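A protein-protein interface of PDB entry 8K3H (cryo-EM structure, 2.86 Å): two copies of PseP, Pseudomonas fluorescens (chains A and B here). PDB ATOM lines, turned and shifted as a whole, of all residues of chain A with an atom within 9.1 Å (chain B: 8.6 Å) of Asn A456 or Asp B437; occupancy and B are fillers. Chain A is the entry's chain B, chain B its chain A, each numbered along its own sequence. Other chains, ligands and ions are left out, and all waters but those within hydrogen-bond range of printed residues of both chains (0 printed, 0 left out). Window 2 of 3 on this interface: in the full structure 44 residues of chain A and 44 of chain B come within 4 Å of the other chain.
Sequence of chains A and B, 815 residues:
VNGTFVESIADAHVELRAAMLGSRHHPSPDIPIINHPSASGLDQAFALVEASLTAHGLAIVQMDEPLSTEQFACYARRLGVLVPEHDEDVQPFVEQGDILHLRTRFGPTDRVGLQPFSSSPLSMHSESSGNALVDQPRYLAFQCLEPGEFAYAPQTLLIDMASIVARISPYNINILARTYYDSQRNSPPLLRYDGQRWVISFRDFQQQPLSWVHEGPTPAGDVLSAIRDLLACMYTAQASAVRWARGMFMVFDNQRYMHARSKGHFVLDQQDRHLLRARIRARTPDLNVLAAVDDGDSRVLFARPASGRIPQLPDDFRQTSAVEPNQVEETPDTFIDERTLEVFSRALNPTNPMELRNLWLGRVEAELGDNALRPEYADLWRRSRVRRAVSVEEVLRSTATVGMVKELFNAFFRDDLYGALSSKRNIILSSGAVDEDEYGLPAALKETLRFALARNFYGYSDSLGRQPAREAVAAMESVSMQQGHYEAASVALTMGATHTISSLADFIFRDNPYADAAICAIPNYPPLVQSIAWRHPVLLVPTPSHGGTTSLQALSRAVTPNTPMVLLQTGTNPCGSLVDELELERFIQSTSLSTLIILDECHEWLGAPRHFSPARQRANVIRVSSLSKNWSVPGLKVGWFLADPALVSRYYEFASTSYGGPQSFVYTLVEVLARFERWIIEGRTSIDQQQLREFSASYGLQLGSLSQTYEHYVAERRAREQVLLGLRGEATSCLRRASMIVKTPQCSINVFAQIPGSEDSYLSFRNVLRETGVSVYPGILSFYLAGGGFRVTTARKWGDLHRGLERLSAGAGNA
OD1 of Asp B437 sits at hydrogen-bond distance from ND2 of Asn A456.
The backbone NH (N) of Leu B441 is in hydrogen-bond range of the side-chain hydroxyl (OH) of Tyr A458, 2.9 Å away.
The side-chain amino group (NZ) of Lys B446 is in hydrogen-bond range of the backbone carbonyl oxygen (O) of Leu A453 (3.2 Å).
NZ of Lys B446 sits at hydrogen-bond distance from OD1 of Asn A456.
N of Gly B635 is in hydrogen-bond range of O of Tyr A458 (2.9 Å).
The side-chain carboxylate (OD1) of Asp B435 lies close to the backbone NH (N) of Asp B437 (3.4 Å).
The side-chain hydroxyl (OG) of Ser B632 sits at hydrogen-bond distance from the backbone carbonyl oxygen (O) of Tyr B439 (3.0 Å).
The side-chain amide oxygen of Asn A456 sits at hydrogen-bond distance from the side-chain hydroxyl of Tyr A458.
The backbone carbonyl oxygen of Gly A459 is in hydrogen-bond range of the side-chain hydroxyl of Ser A664 (2.8 Å).
O of Glu B436 touches CG of Asn A456 (3.5 Å).
Gly B440 touches Tyr A458.
Tyr A458 touches Ser B632 (CE2 to O, 3.1 Å).
CE2 of Tyr A458 touches CG1 of Val B633 (3.5 Å).
Pro B634 touches Tyr A458 (CD to O, 3.2 Å).
CA of Gly A459 touches OE2 of Glu B436 (3.4 Å).
Gly B635 touches Gly A459.
Tyr A460 touches Pro B634.
Ser A664 touches Gly B635 (OG to CA, 3.2 Å).
Phe A665 touches Gly B635.
Asn A456 touches three residues of chain B.
Of the printed residues of chain A, Asp B437 touches Asn A456.
No residue of chain A comes within 4 Å of Glu B438.
Of the printed residues of chain A, Val B633 touches Tyr A458 (3.5 Å).
Printed residues of chain B within 4 Å of Gly A459: Glu B436 and Gly B635.
Of the printed residues of chain A, Pro B634 touches Tyr A458 (3.2 Å) and Tyr A460 (3.4 Å).
Of the printed residues of chain A, Glu B436 touches Asn A456 (3.5 Å) and Gly A459 (3.4 Å).
The nearest residue of chain B that does not touch Asn A456 is Gly B440 (4.9 Å).
The nearest printed residue of chain B that does not touch Phe A665 is Pro B634 (7.1 Å).
Hydrophobic or aromatic side chains of chain B that line the printed part of chain A: Leu B441, Val B633 and Pro B634.
Along chain B the printed residues that touch a printed residue of chain A span positions 436 to 635.
Among the printed residues, 15 pairs touch across the chains.
Among the printed residues, no Asp or Glu carboxylate lies within 4 Å of a Lys or Arg side-chain nitrogen of the other chain.
No position is printed for both chains.
Of the 15 pairs that touch across the chains among the printed residues, none has its exchanged pair printed and touching as well.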
ATOM      1  N   LEU A 449      10.132 -38.091  21.805  1.00  0.00           N
ATOM      2  CA  LEU A 449       9.437 -37.506  22.946  1.00  0.00           C
ATOM      3  C   LEU A 449      10.280 -36.428  23.615  1.00  0.00           C
ATOM      4  O   LEU A 449       9.741 -35.428  24.102  1.00  0.00           O
ATOM      5  CB  LEU A 449       9.060 -38.595  23.949  1.00  0.00           C
ATOM      6  CG  LEU A 449       7.909 -39.507  23.521  1.00  0.00           C
ATOM      7  CD1 LEU A 449       7.576 -40.509  24.612  1.00  0.00           C
ATOM      8  CD2 LEU A 449       6.682 -38.689  23.149  1.00  0.00           C
ATOM      9  N   ARG A 450      11.601 -36.615  23.653  1.00  0.00           N
ATOM     10  CA  ARG A 450      12.479 -35.567  24.160  1.00  0.00           C
ATOM     11  C   ARG A 450      12.545 -34.386  23.202  1.00  0.00           C
ATOM     12  O   ARG A 450      12.746 -33.247  23.635  1.00  0.00           O
ATOM     13  CB  ARG A 450      13.878 -36.129  24.408  1.00  0.00           C
ATOM     14  CG  ARG A 450      14.074 -36.719  25.794  1.00  0.00           C
ATOM     15  CD  ARG A 450      15.395 -37.461  25.895  1.00  0.00           C
ATOM     16  NE  ARG A 450      15.217 -38.906  25.813  1.00  0.00           N
ATOM     17  CZ  ARG A 450      16.041 -39.729  25.177  1.00  0.00           C
ATOM     18  NH1 ARG A 450      17.117 -39.280  24.550  1.00  0.00           N
ATOM     19  NH2 ARG A 450      15.779 -41.032  25.172  1.00  0.00           N
ATOM     20  N   PHE A 451      12.385 -34.639  21.900  1.00  0.00           N
ATOM     21  CA  PHE A 451      12.361 -33.553  20.928  1.00  0.00           C
ATOM     22  C   PHE A 451      11.113 -32.694  21.091  1.00  0.00           C
ATOM     23  O   PHE A 451      11.181 -31.465  20.985  1.00  0.00           O
ATOM     24  CB  PHE A 451      12.450 -34.123  19.512  1.00  0.00           C
ATOM     25  CG  PHE A 451      12.089 -33.140  18.434  1.00  0.00           C
ATOM     26  CD1 PHE A 451      13.011 -32.207  17.993  1.00  0.00           C
ATOM     27  CD2 PHE A 451      10.832 -33.159  17.851  1.00  0.00           C
ATOM     28  CE1 PHE A 451      12.684 -31.306  17.000  1.00  0.00           C
ATOM     29  CE2 PHE A 451      10.500 -32.260  16.857  1.00  0.00           C
ATOM     30  CZ  PHE A 451      11.429 -31.333  16.432  1.00  0.00           C
ATOM     31  N   ALA A 452       9.964 -33.325  21.344  1.00  0.00           N
ATOM     32  CA  ALA A 452       8.740 -32.565  21.573  1.00  0.00           C
ATOM     33  C   ALA A 452       8.824 -31.740  22.850  1.00  0.00           C
ATOM     34  O   ALA A 452       8.263 -30.641  22.915  1.00  0.00           O
ATOM     35  CB  ALA A 452       7.537 -33.507  21.627  1.00  0.00           C
ATOM     36  N   LEU A 453       9.507 -32.257  23.873  1.00  0.00           N
ATOM     37  CA  LEU A 453       9.706 -31.489  25.098  1.00  0.00           C
ATOM     38  C   LEU A 453      10.556 -30.250  24.844  1.00  0.00           C
ATOM     39  O   LEU A 453      10.259 -29.170  25.366  1.00  0.00           O
ATOM     40  CB  LEU A 453      10.351 -32.371  26.166  1.00  0.00           C
ATOM     41  CG  LEU A 453       9.914 -32.149  27.613  1.00  0.00           C
ATOM     42  CD1 LEU A 453       8.408 -32.278  27.744  1.00  0.00           C
ATOM     43  CD2 LEU A 453      10.622 -33.130  28.532  1.00  0.00           C
ATOM     44  N   ALA A 454      11.617 -30.388  24.046  1.00  0.00           N
ATOM     45  CA  ALA A 454      12.503 -29.258  23.787  1.00  0.00           C
ATOM     46  C   ALA A 454      11.831 -28.195  22.930  1.00  0.00           C
ATOM     47  O   ALA A 454      12.114 -27.002  23.090  1.00  0.00           O
ATOM     48  CB  ALA A 454      13.789 -29.742  23.120  1.00  0.00           C
ATOM     49  N   ARG A 455      10.947 -28.598  22.021  1.00  0.00           N
ATOM     50  CA  ARG A 455      10.268 -27.674  21.125  1.00  0.00           C
ATOM     51  C   ARG A 455       8.932 -27.193  21.673  1.00  0.00           C
ATOM     52  O   ARG A 455       8.199 -26.500  20.959  1.00  0.00           O
ATOM     53  CB  ARG A 455      10.063 -28.325  19.754  1.00  0.00           C
ATOM     54  CG  ARG A 455      11.351 -28.579  18.992  1.00  0.00           C
ATOM     55  CD  ARG A 455      11.821 -27.325  18.274  1.00  0.00           C
ATOM     56  NE  ARG A 455      11.194 -27.177  16.966  1.00  0.00           N
ATOM     57  CZ  ARG A 455      11.717 -27.616  15.830  1.00  0.00           C
ATOM     58  NH1 ARG A 455      12.885 -28.237  15.802  1.00  0.00           N
ATOM     59  NH2 ARG A 455      11.052 -27.429  14.694  1.00  0.00           N
ATOM     60  N   ASN A 456       8.604 -27.542  22.920  1.00  0.00           N
ATOM     61  CA  ASN A 456       7.344 -27.148  23.555  1.00  0.00           C
ATOM     62  C   ASN A 456       6.140 -27.590  22.727  1.00  0.00           C
ATOM     63  O   ASN A 456       5.153 -26.863  22.591  1.00  0.00           O
ATOM     64  CB  ASN A 456       7.303 -25.641  23.816  1.00  0.00           C
ATOM     65  CG  ASN A 456       8.498 -25.153  24.610  1.00  0.00           C
ATOM     66  OD1 ASN A 456       8.700 -25.551  25.756  1.00  0.00           O
ATOM     67  ND2 ASN A 456       9.298 -24.287  24.003  1.00  0.00           N
ATOM     68  N   PHE A 457       6.219 -28.800  22.172  1.00  0.00           N
ATOM     69  CA  PHE A 457       5.172 -29.336  21.304  1.00  0.00           C
ATOM     70  C   PHE A 457       4.065 -30.000  22.127  1.00  0.00           C
ATOM     71  O   PHE A 457       3.756 -31.182  21.981  1.00  0.00           O
ATOM     72  CB  PHE A 457       5.777 -30.313  20.304  1.00  0.00           C
ATOM     73  CG  PHE A 457       6.387 -29.653  19.102  1.00  0.00           C
ATOM     74  CD1 PHE A 457       6.068 -28.347  18.774  1.00  0.00           C
ATOM     75  CD2 PHE A 457       7.278 -30.342  18.297  1.00  0.00           C
ATOM     76  CE1 PHE A 457       6.629 -27.740  17.666  1.00  0.00           C
ATOM     77  CE2 PHE A 457       7.842 -29.741  17.189  1.00  0.00           C
ATOM     78  CZ  PHE A 457       7.516 -28.438  16.874  1.00  0.00           C
ATOM     79  N   TYR A 458       3.463 -29.208  23.011  1.00  0.00           N
ATOM     80  CA  TYR A 458       2.363 -29.671  23.855  1.00  0.00           C
ATOM     81  C   TYR A 458       1.262 -28.621  23.943  1.00  0.00           C
ATOM     82  O   TYR A 458       0.713 -28.360  25.019  1.00  0.00           O
ATOM     83  CB  TYR A 458       2.857 -30.070  25.247  1.00  0.00           C
ATOM     84  CG  TYR A 458       3.787 -29.074  25.908  1.00  0.00           C
ATOM     85  CD1 TYR A 458       5.162 -29.259  25.871  1.00  0.00           C
ATOM     86  CD2 TYR A 458       3.298 -27.946  26.549  1.00  0.00           C
ATOM     87  CE1 TYR A 458       6.020 -28.361  26.471  1.00  0.00           C
ATOM     88  CE2 TYR A 458       4.151 -27.036  27.144  1.00  0.00           C
ATOM     89  CZ  TYR A 458       5.511 -27.250  27.103  1.00  0.00           C
ATOM     90  OH  TYR A 458       6.366 -26.351  27.695  1.00  0.00           O
ATOM     91  N   GLY A 459       0.908 -28.015  22.808  1.00  0.00           N
ATOM     92  CA  GLY A 459      -0.192 -27.080  22.743  1.00  0.00           C
ATOM     93  C   GLY A 459      -1.469 -27.724  22.219  1.00  0.00           C
ATOM     94  O   GLY A 459      -1.536 -28.917  21.934  1.00  0.00           O
ATOM     95  N   TYR A 460      -2.505 -26.896  22.103  1.00  0.00           N
ATOM     96  CA  TYR A 460      -3.768 -27.354  21.543  1.00  0.00           C
ATOM     97  C   TYR A 460      -3.602 -27.705  20.067  1.00  0.00           C
ATOM     98  O   TYR A 460      -2.814 -27.092  19.344  1.00  0.00           O
ATOM     99  CB  TYR A 460      -4.852 -26.288  21.704  1.00  0.00           C
ATOM    100  CG  TYR A 460      -5.405 -26.163  23.105  1.00  0.00           C
ATOM    101  CD1 TYR A 460      -6.243 -27.137  23.630  1.00  0.00           C
ATOM    102  CD2 TYR A 460      -5.103 -25.063  23.898  1.00  0.00           C
ATOM    103  CE1 TYR A 460      -6.757 -27.026  24.908  1.00  0.00           C
ATOM    104  CE2 TYR A 460      -5.614 -24.942  25.177  1.00  0.00           C
ATOM    105  CZ  TYR A 460      -6.439 -25.928  25.676  1.00  0.00           C
ATOM    106  OH  TYR A 460      -6.950 -25.816  26.948  1.00  0.00           O
ATOM    107  N   SER A 664      -1.093 -34.026  21.821  1.00  0.00           N
ATOM    108  CA  SER A 664      -0.196 -33.359  20.885  1.00  0.00           C
ATOM    109  C   SER A 664       1.265 -33.626  21.216  1.00  0.00           C
ATOM    110  O   SER A 664       2.131 -33.435  20.356  1.00  0.00           O
ATOM    111  CB  SER A 664      -0.460 -31.852  20.869  1.00  0.00           C
ATOM    112  OG  SER A 664       0.015 -31.235  22.050  1.00  0.00           O
ATOM    113  N   PHE A 665       1.551 -34.073  22.440  1.00  0.00           N
ATOM    114  CA  PHE A 665       2.927 -34.336  22.851  1.00  0.00           C
ATOM    115  C   PHE A 665       3.547 -35.487  22.069  1.00  0.00           C
ATOM    116  O   PHE A 665       4.770 -35.527  21.895  1.00  0.00           O
ATOM    117  CB  PHE A 665       2.962 -34.624  24.353  1.00  0.00           C
ATOM    118  CG  PHE A 665       4.332 -34.923  24.886  1.00  0.00           C
ATOM    119  CD1 PHE A 665       5.306 -33.941  24.918  1.00  0.00           C
ATOM    120  CD2 PHE A 665       4.641 -36.183  25.369  1.00  0.00           C
ATOM    121  CE1 PHE A 665       6.565 -34.212  25.411  1.00  0.00           C
ATOM    122  CE2 PHE A 665       5.899 -36.459  25.865  1.00  0.00           C
ATOM    123  CZ  PHE A 665       6.863 -35.472  25.886  1.00  0.00           C
ATOM    124  N   THR A 668       5.012 -36.195  17.141  1.00  0.00           N
ATOM    125  CA  THR A 668       6.273 -36.529  16.487  1.00  0.00           C
ATOM    126  C   THR A 668       6.550 -38.026  16.555  1.00  0.00           C
ATOM    127  O   THR A 668       7.050 -38.614  15.589  1.00  0.00           O
ATOM    128  CB  THR A 668       7.420 -35.742  17.121  1.00  0.00           C
ATOM    129  OG1 THR A 668       6.999 -34.394  17.360  1.00  0.00           O
ATOM    130  CG2 THR A 668       8.628 -35.731  16.199  1.00  0.00           C
ATOM    131  N   VAL B 434      -1.953 -19.936  27.186  1.00  0.00           N
ATOM    132  CA  VAL B 434      -0.646 -19.317  27.352  1.00  0.00           C
ATOM    133  C   VAL B 434       0.302 -19.824  26.274  1.00  0.00           C
ATOM    134  O   VAL B 434       0.285 -21.008  25.911  1.00  0.00           O
ATOM    135  CB  VAL B 434      -0.096 -19.603  28.760  1.00  0.00           C
ATOM    136  CG1 VAL B 434       1.167 -18.799  29.015  1.00  0.00           C
ATOM    137  CG2 VAL B 434      -1.149 -19.299  29.812  1.00  0.00           C
ATOM    138  N   ASP B 435       1.131 -18.922  25.748  1.00  0.00           N
ATOM    139  CA  ASP B 435       2.100 -19.279  24.719  1.00  0.00           C
ATOM    140  C   ASP B 435       3.098 -20.296  25.257  1.00  0.00           C
ATOM    141  O   ASP B 435       3.919 -19.974  26.121  1.00  0.00           O
ATOM    142  CB  ASP B 435       2.826 -18.031  24.213  1.00  0.00           C
ATOM    143  CG  ASP B 435       3.520 -18.258  22.885  1.00  0.00           C
ATOM    144  OD1 ASP B 435       3.444 -19.386  22.353  1.00  0.00           O
ATOM    145  OD2 ASP B 435       4.142 -17.305  22.368  1.00  0.00           O
ATOM    146  N   GLU B 436       3.031 -21.529  24.749  1.00  0.00           N
ATOM    147  CA  GLU B 436       3.912 -22.584  25.236  1.00  0.00           C
ATOM    148  C   GLU B 436       5.366 -22.325  24.867  1.00  0.00           C
ATOM    149  O   GLU B 436       6.271 -22.701  25.621  1.00  0.00           O
ATOM    150  CB  GLU B 436       3.462 -23.937  24.687  1.00  0.00           C
ATOM    151  CG  GLU B 436       2.029 -24.303  25.036  1.00  0.00           C
ATOM    152  CD  GLU B 436       1.048 -23.942  23.938  1.00  0.00           C
ATOM    153  OE1 GLU B 436       1.497 -23.639  22.813  1.00  0.00           O
ATOM    154  OE2 GLU B 436      -0.172 -23.960  24.200  1.00  0.00           O
ATOM    155  N   ASP B 437       5.613 -21.689  23.721  1.00  0.00           N
ATOM    156  CA  ASP B 437       6.986 -21.466  23.284  1.00  0.00           C
ATOM    157  C   ASP B 437       7.655 -20.364  24.096  1.00  0.00           C
ATOM    158  O   ASP B 437       8.882 -20.359  24.252  1.00  0.00           O
ATOM    159  CB  ASP B 437       7.012 -21.130  21.794  1.00  0.00           C
ATOM    160  CG  ASP B 437       8.270 -21.624  21.109  1.00  0.00           C
ATOM    161  OD1 ASP B 437       9.124 -22.226  21.793  1.00  0.00           O
ATOM    162  OD2 ASP B 437       8.404 -21.412  19.886  1.00  0.00           O
ATOM    163  N   GLU B 438       6.871 -19.425  24.622  1.00  0.00           N
ATOM    164  CA  GLU B 438       7.418 -18.320  25.399  1.00  0.00           C
ATOM    165  C   GLU B 438       7.263 -18.542  26.900  1.00  0.00           C
ATOM    166  O   GLU B 438       8.211 -18.331  27.662  1.00  0.00           O
ATOM    167  CB  GLU B 438       6.747 -17.006  24.986  1.00  0.00           C
ATOM    168  N   TYR B 439       6.080 -18.964  27.338  1.00  0.00           N
ATOM    169  CA  TYR B 439       5.795 -19.220  28.748  1.00  0.00           C
ATOM    170  C   TYR B 439       5.331 -20.670  28.846  1.00  0.00           C
ATOM    171  O   TYR B 439       4.131 -20.953  28.816  1.00  0.00           O
ATOM    172  CB  TYR B 439       4.736 -18.255  29.276  1.00  0.00           C
ATOM    173  CG  TYR B 439       4.994 -16.806  28.929  1.00  0.00           C
ATOM    174  CD1 TYR B 439       6.016 -16.093  29.540  1.00  0.00           C
ATOM    175  CD2 TYR B 439       4.215 -16.153  27.984  1.00  0.00           C
ATOM    176  CE1 TYR B 439       6.252 -14.769  29.219  1.00  0.00           C
ATOM    177  CE2 TYR B 439       4.444 -14.832  27.657  1.00  0.00           C
ATOM    178  CZ  TYR B 439       5.463 -14.145  28.276  1.00  0.00           C
ATOM    179  OH  TYR B 439       5.691 -12.827  27.951  1.00  0.00           O
ATOM    180  N   GLY B 440       6.286 -21.591  28.982  1.00  0.00           N
ATOM    181  CA  GLY B 440       6.012 -23.002  28.946  1.00  0.00           C
ATOM    182  C   GLY B 440       6.146 -23.672  30.296  1.00  0.00           C
ATOM    183  O   GLY B 440       6.146 -23.024  31.353  1.00  0.00           O
ATOM    184  N   LEU B 441       6.252 -24.995  30.263  1.00  0.00           N
ATOM    185  CA  LEU B 441       6.422 -25.768  31.482  1.00  0.00           C
ATOM    186  C   LEU B 441       7.784 -25.468  32.106  1.00  0.00           C
ATOM    187  O   LEU B 441       8.781 -25.342  31.387  1.00  0.00           O
ATOM    188  CB  LEU B 441       6.297 -27.261  31.183  1.00  0.00           C
ATOM    189  CG  LEU B 441       6.069 -28.220  32.352  1.00  0.00           C
ATOM    190  CD1 LEU B 441       4.728 -27.956  33.015  1.00  0.00           C
ATOM    191  CD2 LEU B 441       6.159 -29.660  31.879  1.00  0.00           C
ATOM    192  N   PRO B 442       7.858 -25.333  33.430  1.00  0.00           N
ATOM    193  CA  PRO B 442       9.152 -25.081  34.070  1.00  0.00           C
ATOM    194  C   PRO B 442      10.118 -26.236  33.851  1.00  0.00           C
ATOM    195  O   PRO B 442       9.716 -27.391  33.697  1.00  0.00           O
ATOM    196  CB  PRO B 442       8.789 -24.926  35.552  1.00  0.00           C
ATOM    197  CG  PRO B 442       7.348 -24.534  35.544  1.00  0.00           C
ATOM    198  CD  PRO B 442       6.751 -25.289  34.398  1.00  0.00           C
ATOM    199  N   ALA B 443      11.411 -25.903  33.831  1.00  0.00           N
ATOM    200  CA  ALA B 443      12.437 -26.908  33.571  1.00  0.00           C
ATOM    201  C   ALA B 443      12.430 -28.011  34.620  1.00  0.00           C
ATOM    202  O   ALA B 443      12.785 -29.156  34.317  1.00  0.00           O
ATOM    203  CB  ALA B 443      13.814 -26.247  33.504  1.00  0.00           C
ATOM    204  N   LYS B 446       9.743 -30.322  33.436  1.00  0.00           N
ATOM    205  CA  LYS B 446      10.159 -31.010  32.219  1.00  0.00           C
ATOM    206  C   LYS B 446      11.221 -32.060  32.509  1.00  0.00           C
ATOM    207  O   LYS B 446      11.363 -33.024  31.748  1.00  0.00           O
ATOM    208  CB  LYS B 446      10.673 -30.003  31.191  1.00  0.00           C
ATOM    209  CG  LYS B 446       9.579 -29.197  30.512  1.00  0.00           C
ATOM    210  CD  LYS B 446      10.138 -27.966  29.819  1.00  0.00           C
ATOM    211  CE  LYS B 446      10.787 -28.324  28.496  1.00  0.00           C
ATOM    212  NZ  LYS B 446      11.037 -27.118  27.661  1.00  0.00           N
ATOM    213  N   SER B 632       0.253 -24.359  31.401  1.00  0.00           N
ATOM    214  CA  SER B 632       0.394 -24.226  29.951  1.00  0.00           C
ATOM    215  C   SER B 632       0.879 -25.525  29.305  1.00  0.00           C
ATOM    216  O   SER B 632       1.818 -25.545  28.509  1.00  0.00           O
ATOM    217  CB  SER B 632       1.320 -23.058  29.597  1.00  0.00           C
ATOM    218  OG  SER B 632       2.663 -23.335  29.951  1.00  0.00           O
ATOM    219  N   VAL B 633       0.212 -26.621  29.657  1.00  0.00           N
ATOM    220  CA  VAL B 633       0.457 -27.908  29.007  1.00  0.00           C
ATOM    221  C   VAL B 633      -0.866 -28.537  28.577  1.00  0.00           C
ATOM    222  O   VAL B 633      -1.243 -29.605  29.081  1.00  0.00           O
ATOM    223  CB  VAL B 633       1.271 -28.847  29.916  1.00  0.00           C
ATOM    224  CG1 VAL B 633       2.690 -28.340  30.055  1.00  0.00           C
ATOM    225  CG2 VAL B 633       0.649 -28.939  31.300  1.00  0.00           C
ATOM    226  N   PRO B 634      -1.598 -27.926  27.637  1.00  0.00           N
ATOM    227  CA  PRO B 634      -2.838 -28.555  27.155  1.00  0.00           C
ATOM    228  C   PRO B 634      -2.615 -29.873  26.439  1.00  0.00           C
ATOM    229  O   PRO B 634      -3.488 -30.747  26.500  1.00  0.00           O
ATOM    230  CB  PRO B 634      -3.427 -27.502  26.204  1.00  0.00           C
ATOM    231  CG  PRO B 634      -2.617 -26.258  26.412  1.00  0.00           C
ATOM    232  CD  PRO B 634      -1.281 -26.700  26.890  1.00  0.00           C
ATOM    233  N   GLY B 635      -1.479 -30.045  25.762  1.00  0.00           N
ATOM    234  CA  GLY B 635      -1.218 -31.258  25.013  1.00  0.00           C
ATOM    235  C   GLY B 635      -0.782 -32.444  25.838  1.00  0.00           C
ATOM    236  O   GLY B 635      -0.642 -33.542  25.291  1.00  0.00           O
ATOM    237  N   ALA B 795      -1.767 -13.401  27.024  1.00  0.00           N
ATOM    238  CA  ALA B 795      -0.636 -14.251  27.395  1.00  0.00           C
ATOM    239  C   ALA B 795       0.119 -14.755  26.169  1.00  0.00           C
ATOM    240  O   ALA B 795       0.339 -15.952  25.994  1.00  0.00           O
ATOM    241  CB  ALA B 795      -1.117 -15.412  28.256  1.00  0.00           C
ATOM    242  N   ARG B 796       0.524 -13.830  25.310  1.00  0.00           N
ATOM    243  CA  ARG B 796       1.279 -14.132  24.103  1.00  0.00           C
ATOM    244  C   ARG B 796       2.665 -13.504  24.203  1.00  0.00           C
ATOM    245  O   ARG B 796       2.994 -12.821  25.175  1.00  0.00           O
ATOM    246  CB  ARG B 796       0.540 -13.632  22.858  1.00  0.00           C
ATOM    247  CG  ARG B 796      -0.969 -13.779  22.929  1.00  0.00           C
ATOM    248  CD  ARG B 796      -1.380 -15.239  22.897  1.00  0.00           C
ATOM    249  NE  ARG B 796      -0.621 -15.994  21.909  1.00  0.00           N
ATOM    250  CZ  ARG B 796      -0.486 -17.313  21.914  1.00  0.00           C
ATOM    251  NH1 ARG B 796      -1.050 -18.061  22.848  1.00  0.00           N
ATOM    252  NH2 ARG B 796       0.231 -17.895  20.958  1.00  0.00           N
ATOM    253  N   LYS B 797       3.484 -13.753  23.187  1.00  0.00           N
ATOM    254  CA  LYS B 797       4.778 -13.094  23.100  1.00  0.00           C
ATOM    255  C   LYS B 797       4.583 -11.592  22.950  1.00  0.00           C
ATOM    256  O   LYS B 797       3.637 -11.136  22.303  1.00  0.00           O
ATOM    257  CB  LYS B 797       5.583 -13.645  21.924  1.00  0.00           C
